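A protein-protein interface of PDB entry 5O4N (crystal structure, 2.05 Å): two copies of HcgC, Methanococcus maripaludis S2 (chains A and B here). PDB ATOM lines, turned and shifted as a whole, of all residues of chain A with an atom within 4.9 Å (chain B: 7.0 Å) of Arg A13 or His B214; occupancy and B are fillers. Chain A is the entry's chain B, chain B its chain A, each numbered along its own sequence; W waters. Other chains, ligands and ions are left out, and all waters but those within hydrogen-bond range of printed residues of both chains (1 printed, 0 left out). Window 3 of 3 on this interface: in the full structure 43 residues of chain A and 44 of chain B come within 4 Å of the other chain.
The side-chain hydroxyl (OH) of Tyr B207 is in hydrogen-bond range of the side-chain hydroxyl (OG1) of Thr A11 (2.7 Å).
The backbone carbonyl oxygen of Tyr A3 lies within hydrogen-bond range of a ring nitrogen (NE2) of His B214 (2.9 Å).
NE2 of His B214 lies within hydrogen-bond range of O of Gly A4 (3.4 Å).
O of Asn A2 sits at hydrogen-bond distance from N of Thr A11, at 2.8 Å.
OE2 of Glu B209 lies within hydrogen-bond range of OH of Tyr B207 (2.7 Å).
Among the printed residues, pairs that only touch across the chains: Gly A4 with Glu B209, Gly A4 with Tyr B207, Arg A13 with His B214, Arg A13 with Tyr B207 and Thr A231 with Tyr B207.
Printed residues of chain B within 4 Å of Arg A13: Tyr B207 (3.8 Å) and His B214 (3.8 Å).
Of chain A, only Tyr A3, Gly A4 and Arg A13 come within 4 Å of His B214.
Printed residues of chain A within 4 Å of Glu B209: Gly A4.
Printed residues of chain B within 4 Å of Thr A231: Tyr B207.
Printed residues of chain A within 4 Å of Tyr B207: Gly A4, Thr A11, Arg A13 and Thr A231.
Printed residues of chain B within 4 Å of Gly A4: Tyr B207, Glu B209 and His B214.
Of the printed residues of chain B, Thr A11 touches Tyr B207.
Gly B210 touches none of the printed residues of chain A.
Lys B216 touches none of the printed residues of chain A.
The nearest residue of chain A that does not touch His B214 is Thr A11 (4.5 Å).
Printed residues of chain A that touch a printed residue of chain B: Tyr A3, Gly A4, Thr A11, Arg A13 and Thr A231.
Among the printed residues, 8 pairs touch across the chains.
No position is printed for both chains.
Of the 8 pairs that touch across the chains among the printed residues, none has its exchanged pair printed and touching as well.
Water W1 lies within hydrogen-bond range of OG1 of Thr A11 (2.7 Å) and OE2 of Glu B209 (2.9 Å).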
ATOM      1  N   MET A   1      -8.469  23.034 -19.079  1.00  0.00           N
ATOM      2  CA  MET A   1      -7.934  23.363 -20.402  1.00  0.00           C
ATOM      3  C   MET A   1      -6.909  24.499 -20.360  1.00  0.00           C
ATOM      4  O   MET A   1      -6.698  25.137 -19.330  1.00  0.00           O
ATOM      5  CB  MET A   1      -9.090  23.681 -21.382  1.00  0.00           C
ATOM      6  CG  MET A   1      -9.711  25.065 -21.218  1.00  0.00           C
ATOM      7  SD  MET A   1      -9.600  26.033 -22.750  1.00  0.00           S
ATOM      8  CE  MET A   1      -8.752  27.477 -22.166  1.00  0.00           C
ATOM      9  N   ASN A   2      -6.278  24.727 -21.496  1.00  0.00           N
ATOM     10  CA  ASN A   2      -5.272  25.760 -21.700  1.00  0.00           C
ATOM     11  C   ASN A   2      -5.496  26.311 -23.126  1.00  0.00           C
ATOM     12  O   ASN A   2      -6.450  25.927 -23.797  1.00  0.00           O
ATOM     13  CB  ASN A   2      -3.854  25.141 -21.556  1.00  0.00           C
ATOM     14  CG  ASN A   2      -3.439  24.816 -20.137  1.00  0.00           C
ATOM     15  OD1 ASN A   2      -3.703  25.571 -19.197  1.00  0.00           O
ATOM     16  ND2 ASN A   2      -2.654  23.757 -19.963  1.00  0.00           N
ATOM     17  N   TYR A   3      -4.632  27.195 -23.571  1.00  0.00           N
ATOM     18  CA  TYR A   3      -4.694  27.786 -24.893  1.00  0.00           C
ATOM     19  C   TYR A   3      -3.678  27.063 -25.736  1.00  0.00           C
ATOM     20  O   TYR A   3      -2.852  26.325 -25.195  1.00  0.00           O
ATOM     21  CB  TYR A   3      -4.411  29.291 -24.836  1.00  0.00           C
ATOM     22  CG  TYR A   3      -5.547  30.093 -24.237  1.00  0.00           C
ATOM     23  CD1 TYR A   3      -6.862  29.913 -24.677  1.00  0.00           C
ATOM     24  CD2 TYR A   3      -5.316  31.044 -23.256  1.00  0.00           C
ATOM     25  CE1 TYR A   3      -7.908  30.649 -24.137  1.00  0.00           C
ATOM     26  CE2 TYR A   3      -6.355  31.792 -22.710  1.00  0.00           C
ATOM     27  CZ  TYR A   3      -7.655  31.589 -23.151  1.00  0.00           C
ATOM     28  OH  TYR A   3      -8.704  32.316 -22.620  1.00  0.00           O
ATOM     29  N   GLY A   4      -3.752  27.260 -27.042  1.00  0.00           N
ATOM     30  CA  GLY A   4      -2.832  26.621 -27.973  1.00  0.00           C
ATOM     31  C   GLY A   4      -1.702  27.560 -28.349  1.00  0.00           C
ATOM     32  O   GLY A   4      -0.943  28.001 -27.484  1.00  0.00           O
ATOM     33  N   THR A  11      -7.058  24.480 -26.129  1.00  0.00           N
ATOM     34  CA  THR A  11      -6.553  23.119 -26.155  1.00  0.00           C
ATOM     35  C   THR A  11      -7.265  22.429 -25.012  1.00  0.00           C
ATOM     36  O   THR A  11      -7.134  22.875 -23.889  1.00  0.00           O
ATOM     37  CB  THR A  11      -5.050  23.015 -25.994  1.00  0.00           C
ATOM     38  OG1 THR A  11      -4.434  23.658 -27.104  1.00  0.00           O
ATOM     39  CG2 THR A  11      -4.602  21.574 -25.931  1.00  0.00           C
ATOM     40  N   THR A  12      -7.998  21.355 -25.282  1.00  0.00           N
ATOM     41  CA  THR A  12      -8.743  20.617 -24.274  1.00  0.00           C
ATOM     42  C   THR A  12      -8.342  19.165 -24.269  1.00  0.00           C
ATOM     43  O   THR A  12      -8.413  18.518 -25.299  1.00  0.00           O
ATOM     44  CB  THR A  12     -10.241  20.762 -24.591  1.00  0.00           C
ATOM     45  OG1 THR A  12     -10.518  22.151 -24.777  1.00  0.00           O
ATOM     46  CG2 THR A  12     -11.135  20.122 -23.554  1.00  0.00           C
ATOM     47  N   ARG A  13      -7.949  18.650 -23.104  1.00  0.00           N
ATOM     48  CA  ARG A  13      -7.554  17.261 -22.946  1.00  0.00           C
ATOM     49  C   ARG A  13      -8.719  16.598 -22.234  1.00  0.00           C
ATOM     50  O   ARG A  13      -9.214  17.159 -21.275  1.00  0.00           O
ATOM     51  CB  ARG A  13      -6.264  17.174 -22.145  1.00  0.00           C
ATOM     52  CG  ARG A  13      -5.091  17.863 -22.882  1.00  0.00           C
ATOM     53  CD  ARG A  13      -3.956  18.217 -21.957  1.00  0.00           C
ATOM     54  NE  ARG A  13      -3.004  19.149 -22.572  1.00  0.00           N
ATOM     55  CZ  ARG A  13      -3.171  20.467 -22.715  1.00  0.00           C
ATOM     56  NH1 ARG A  13      -2.230  21.203 -23.285  1.00  0.00           N
ATOM     57  NH2 ARG A  13      -4.288  21.058 -22.288  1.00  0.00           N
ATOM     58  N   SER A  14      -9.168  15.429 -22.693  1.00  0.00           N
ATOM     59  CA  SER A  14     -10.284  14.731 -22.070  1.00  0.00           C
ATOM     60  C   SER A  14      -9.952  14.300 -20.661  1.00  0.00           C
ATOM     61  O   SER A  14      -8.800  13.929 -20.368  1.00  0.00           O
ATOM     62  CB  SER A  14     -10.704  13.512 -22.912  1.00  0.00           C
ATOM     63  OG  SER A  14      -9.689  12.534 -23.047  1.00  0.00           O
ATOM     64  N   LYS A  15     -10.968  14.384 -19.776  1.00  0.00           N
ATOM     65  CA  LYS A  15     -10.868  13.986 -18.365  1.00  0.00           C
ATOM     66  C   LYS A  15     -10.793  12.456 -18.403  1.00  0.00           C
ATOM     67  O   LYS A  15     -10.135  11.848 -17.567  1.00  0.00           O
ATOM     68  CB  LYS A  15     -12.077  14.466 -17.544  1.00  0.00           C
ATOM     69  CG  LYS A  15     -12.184  15.986 -17.428  1.00  0.00           C
ATOM     70  CD  LYS A  15     -11.190  16.623 -16.447  1.00  0.00           C
ATOM     71  CE  LYS A  15     -10.720  18.000 -16.887  1.00  0.00           C
ATOM     72  NZ  LYS A  15     -11.842  18.971 -17.025  1.00  0.00           N
ATOM     73  N   SER A 228      -4.666  11.331 -21.333  1.00  0.00           N
ATOM     74  CA  SER A 228      -6.021  11.704 -21.739  1.00  0.00           C
ATOM     75  C   SER A 228      -6.225  10.952 -23.027  1.00  0.00           C
ATOM     76  O   SER A 228      -5.286  10.884 -23.834  1.00  0.00           O
ATOM     77  CB  SER A 228      -6.111  13.185 -22.093  1.00  0.00           C
ATOM     78  OG  SER A 228      -6.011  13.973 -20.925  1.00  0.00           O
ATOM     79  N   ILE A 230      -8.191  11.799 -25.556  1.00  0.00           N
ATOM     80  CA  ILE A 230      -8.220  12.720 -26.693  1.00  0.00           C
ATOM     81  C   ILE A 230      -7.808  14.135 -26.319  1.00  0.00           C
ATOM     82  O   ILE A 230      -8.095  14.603 -25.229  1.00  0.00           O
ATOM     83  CB  ILE A 230      -9.678  12.707 -27.315  1.00  0.00           C
ATOM     84  CG1 ILE A 230      -9.995  11.360 -28.013  1.00  0.00           C
ATOM     85  CG2 ILE A 230      -9.915  13.880 -28.315  1.00  0.00           C
ATOM     86  CD1 ILE A 230     -11.441  11.162 -28.383  1.00  0.00           C
ATOM     87  N   THR A 231      -7.145  14.827 -27.271  1.00  0.00           N
ATOM     88  CA  THR A 231      -6.726  16.206 -27.125  1.00  0.00           C
ATOM     89  C   THR A 231      -7.397  16.929 -28.292  1.00  0.00           C
ATOM     90  O   THR A 231      -7.312  16.485 -29.422  1.00  0.00           O
ATOM     91  CB  THR A 231      -5.211  16.385 -27.002  1.00  0.00           C
ATOM     92  OG1 THR A 231      -4.797  15.671 -25.830  1.00  0.00           O
ATOM     93  CG2 THR A 231      -4.819  17.860 -26.837  1.00  0.00           C
ATOM     94  N   LEU A 242     -16.901  16.527 -25.598  1.00  0.00           N
ATOM     95  CA  LEU A 242     -15.749  15.654 -25.600  1.00  0.00           C
ATOM     96  C   LEU A 242     -16.045  14.409 -24.709  1.00  0.00           C
ATOM     97  O   LEU A 242     -15.997  13.275 -25.198  1.00  0.00           O
ATOM     98  CB  LEU A 242     -14.524  16.434 -25.091  1.00  0.00           C
ATOM     99  CG  LEU A 242     -13.187  15.691 -24.947  1.00  0.00           C
ATOM    100  CD1 LEU A 242     -12.879  14.840 -26.159  1.00  0.00           C
ATOM    101  CD2 LEU A 242     -12.060  16.668 -24.723  1.00  0.00           C
ATOM    102  N   GLU A 243     -16.379  14.627 -23.441  1.00  0.00           N
ATOM    103  CA  GLU A 243     -16.681  13.516 -22.508  1.00  0.00           C
ATOM    104  C   GLU A 243     -17.933  12.781 -22.886  1.00  0.00           C
ATOM    105  O   GLU A 243     -17.952  11.563 -22.789  1.00  0.00           O
ATOM    106  CB  GLU A 243     -16.860  14.000 -21.046  1.00  0.00           C
ATOM    107  CG  GLU A 243     -15.694  14.769 -20.458  1.00  0.00           C
ATOM    108  CD  GLU A 243     -14.316  14.211 -20.753  1.00  0.00           C
ATOM    109  OE1 GLU A 243     -14.110  12.986 -20.620  1.00  0.00           O
ATOM    110  OE2 GLU A 243     -13.408  15.021 -21.025  1.00  0.00           O
ATOM    111  N   GLN B  74       6.960  34.329 -30.885  1.00  0.00           N
ATOM    112  CA  GLN B  74       7.690  33.431 -29.987  1.00  0.00           C
ATOM    113  C   GLN B  74       9.213  33.415 -30.353  1.00  0.00           C
ATOM    114  O   GLN B  74       9.594  32.821 -31.369  1.00  0.00           O
ATOM    115  CB  GLN B  74       7.146  32.003 -30.114  1.00  0.00           C
ATOM    116  CG  GLN B  74       5.665  31.850 -29.829  1.00  0.00           C
ATOM    117  CD  GLN B  74       5.311  31.756 -28.371  1.00  0.00           C
ATOM    118  OE1 GLN B  74       6.133  31.980 -27.476  1.00  0.00           O
ATOM    119  NE2 GLN B  74       4.049  31.415 -28.110  1.00  0.00           N
ATOM    120  N   HIS B  76      11.747  31.632 -29.252  1.00  0.00           N
ATOM    121  CA  HIS B  76      12.333  30.289 -29.305  1.00  0.00           C
ATOM    122  C   HIS B  76      12.155  29.602 -30.674  1.00  0.00           C
ATOM    123  O   HIS B  76      12.897  28.671 -30.978  1.00  0.00           O
ATOM    124  CB  HIS B  76      11.836  29.410 -28.157  1.00  0.00           C
ATOM    125  CG  HIS B  76      10.467  28.858 -28.391  1.00  0.00           C
ATOM    126  ND1 HIS B  76       9.342  29.635 -28.225  1.00  0.00           N
ATOM    127  CD2 HIS B  76      10.095  27.621 -28.788  1.00  0.00           C
ATOM    128  CE1 HIS B  76       8.321  28.850 -28.515  1.00  0.00           C
ATOM    129  NE2 HIS B  76       8.729  27.627 -28.851  1.00  0.00           N
ATOM    130  N   TYR B 207      -0.222  15.517 -29.145  1.00  0.00           N
ATOM    131  CA  TYR B 207      -0.375  16.960 -29.268  1.00  0.00           C
ATOM    132  C   TYR B 207       1.034  17.589 -29.489  1.00  0.00           C
ATOM    133  O   TYR B 207       1.630  18.186 -28.591  1.00  0.00           O
ATOM    134  CB  TYR B 207      -1.115  17.481 -28.023  1.00  0.00           C
ATOM    135  CG  TYR B 207      -1.326  18.969 -27.999  1.00  0.00           C
ATOM    136  CD1 TYR B 207      -1.969  19.623 -29.048  1.00  0.00           C
ATOM    137  CD2 TYR B 207      -0.879  19.730 -26.935  1.00  0.00           C
ATOM    138  CE1 TYR B 207      -2.169  20.997 -29.027  1.00  0.00           C
ATOM    139  CE2 TYR B 207      -1.062  21.103 -26.906  1.00  0.00           C
ATOM    140  CZ  TYR B 207      -1.701  21.739 -27.961  1.00  0.00           C
ATOM    141  OH  TYR B 207      -1.881  23.106 -27.910  1.00  0.00           O
ATOM    142  N   GLU B 209       1.886  20.177 -31.166  1.00  0.00           N
ATOM    143  CA  GLU B 209       1.838  21.631 -31.010  1.00  0.00           C
ATOM    144  C   GLU B 209       2.258  22.000 -29.562  1.00  0.00           C
ATOM    145  O   GLU B 209       2.952  22.988 -29.362  1.00  0.00           O
ATOM    146  CB  GLU B 209       0.418  22.123 -31.363  1.00  0.00           C
ATOM    147  CG  GLU B 209       0.115  23.593 -31.129  1.00  0.00           C
ATOM    148  CD  GLU B 209      -1.361  23.886 -31.316  1.00  0.00           C
ATOM    149  OE1 GLU B 209      -1.862  23.615 -32.427  1.00  0.00           O
ATOM    150  OE2 GLU B 209      -2.038  24.294 -30.340  1.00  0.00           O
ATOM    151  N   GLY B 210       1.852  21.186 -28.587  1.00  0.00           N
ATOM    152  CA  GLY B 210       2.199  21.384 -27.189  1.00  0.00           C
ATOM    153  C   GLY B 210       3.707  21.342 -26.947  1.00  0.00           C
ATOM    154  O   GLY B 210       4.234  22.126 -26.166  1.00  0.00           O
ATOM    155  N   THR B 211       4.422  20.435 -27.632  1.00  0.00           N
ATOM    156  CA  THR B 211       5.867  20.324 -27.492  1.00  0.00           C
ATOM    157  C   THR B 211       6.557  21.604 -27.962  1.00  0.00           C
ATOM    158  O   THR B 211       7.536  22.031 -27.368  1.00  0.00           O
ATOM    159  CB  THR B 211       6.390  19.121 -28.307  1.00  0.00           C
ATOM    160  OG1 THR B 211       5.572  17.992 -28.017  1.00  0.00           O
ATOM    161  CG2 THR B 211       7.854  18.800 -28.000  1.00  0.00           C
ATOM    162  N   VAL B 212       6.035  22.213 -29.027  1.00  0.00           N
ATOM    163  CA  VAL B 212       6.606  23.428 -29.577  1.00  0.00           C
ATOM    164  C   VAL B 212       6.252  24.681 -28.784  1.00  0.00           C
ATOM    165  O   VAL B 212       7.125  25.474 -28.493  1.00  0.00           O
ATOM    166  CB  VAL B 212       6.167  23.623 -31.057  1.00  0.00           C
ATOM    167  CG1 VAL B 212       6.711  24.931 -31.630  1.00  0.00           C
ATOM    168  CG2 VAL B 212       6.591  22.460 -31.918  1.00  0.00           C
ATOM    169  N   PHE B 213       4.998  24.879 -28.479  1.00  0.00           N
ATOM    170  CA  PHE B 213       4.530  26.101 -27.785  1.00  0.00           C
ATOM    171  C   PHE B 213       4.399  26.074 -26.265  1.00  0.00           C
ATOM    172  O   PHE B 213       4.465  27.146 -25.662  1.00  0.00           O
ATOM    173  CB  PHE B 213       3.185  26.495 -28.404  1.00  0.00           C
ATOM    174  CG  PHE B 213       3.394  26.895 -29.838  1.00  0.00           C
ATOM    175  CD1 PHE B 213       3.247  25.969 -30.867  1.00  0.00           C
ATOM    176  CD2 PHE B 213       3.802  28.177 -30.164  1.00  0.00           C
ATOM    177  CE1 PHE B 213       3.492  26.324 -32.187  1.00  0.00           C
ATOM    178  CE2 PHE B 213       4.029  28.532 -31.492  1.00  0.00           C
ATOM    179  CZ  PHE B 213       3.870  27.605 -32.493  1.00  0.00           C
ATOM    180  N   HIS B 214       4.194  24.916 -25.649  1.00  0.00           N
ATOM    181  CA  HIS B 214       4.052  24.828 -24.194  1.00  0.00           C
ATOM    182  C   HIS B 214       5.379  24.393 -23.574  1.00  0.00           C
ATOM    183  O   HIS B 214       5.810  24.984 -22.588  1.00  0.00           O
ATOM    184  CB  HIS B 214       2.881  23.920 -23.806  1.00  0.00           C
ATOM    185  CG  HIS B 214       1.570  24.378 -24.385  1.00  0.00           C
ATOM    186  ND1 HIS B 214       0.477  23.525 -24.473  1.00  0.00           N
ATOM    187  CD2 HIS B 214       1.214  25.590 -24.889  1.00  0.00           C
ATOM    188  CE1 HIS B 214      -0.491  24.239 -25.026  1.00  0.00           C
ATOM    189  NE2 HIS B 214      -0.092  25.485 -25.289  1.00  0.00           N
ATOM    190  N   GLU B 215       6.037  23.381 -24.147  1.00  0.00           N
ATOM    191  CA  GLU B 215       7.325  22.932 -23.619  1.00  0.00           C
ATOM    192  C   GLU B 215       8.438  23.755 -24.248  1.00  0.00           C
ATOM    193  O   GLU B 215       9.582  23.658 -23.791  1.00  0.00           O
ATOM    194  CB  GLU B 215       7.547  21.429 -23.895  1.00  0.00           C
ATOM    195  CG  GLU B 215       6.625  20.539 -23.078  1.00  0.00           C
ATOM    196  CD  GLU B 215       6.433  19.152 -23.658  1.00  0.00           C
ATOM    197  OE1 GLU B 215       5.280  18.661 -23.657  1.00  0.00           O
ATOM    198  OE2 GLU B 215       7.433  18.562 -24.125  1.00  0.00           O
ATOM    199  N   LYS B 216       8.123  24.565 -25.311  1.00  0.00           N
ATOM    200  CA  LYS B 216       9.105  25.407 -25.997  1.00  0.00           C
ATOM    201  C   LYS B 216      10.333  24.580 -26.389  1.00  0.00           C
ATOM    202  O   LYS B 216      11.457  25.021 -26.195  1.00  0.00           O
ATOM    203  CB  LYS B 216       9.452  26.604 -25.098  1.00  0.00           C
ATOM    204  CG  LYS B 216       8.244  27.483 -24.846  1.00  0.00           C
ATOM    205  CD  LYS B 216       8.572  28.703 -23.992  1.00  0.00           C
ATOM    206  CE  LYS B 216       7.810  29.940 -24.415  1.00  0.00           C
ATOM    207  NZ  LYS B 216       6.333  29.775 -24.311  1.00  0.00           N
ATOM    208  N   ASN B 217      10.099  23.363 -26.933  1.00  0.00           N
ATOM    209  CA  ASN B 217      11.173  22.433 -27.319  1.00  0.00           C
ATOM    210  C   ASN B 217      11.068  21.975 -28.766  1.00  0.00           C
ATOM    211  O   ASN B 217      10.476  20.943 -29.051  1.00  0.00           O
ATOM    212  CB  ASN B 217      11.113  21.249 -26.342  1.00  0.00           C
ATOM    213  CG  ASN B 217      12.343  20.388 -26.312  1.00  0.00           C
ATOM    214  OD1 ASN B 217      13.161  20.402 -27.220  1.00  0.00           O
ATOM    215  ND2 ASN B 217      12.445  19.549 -25.303  1.00  0.00           N
HETATM  216  O   HOH W   1      -4.858  24.265 -29.681  1.00  0.00           O
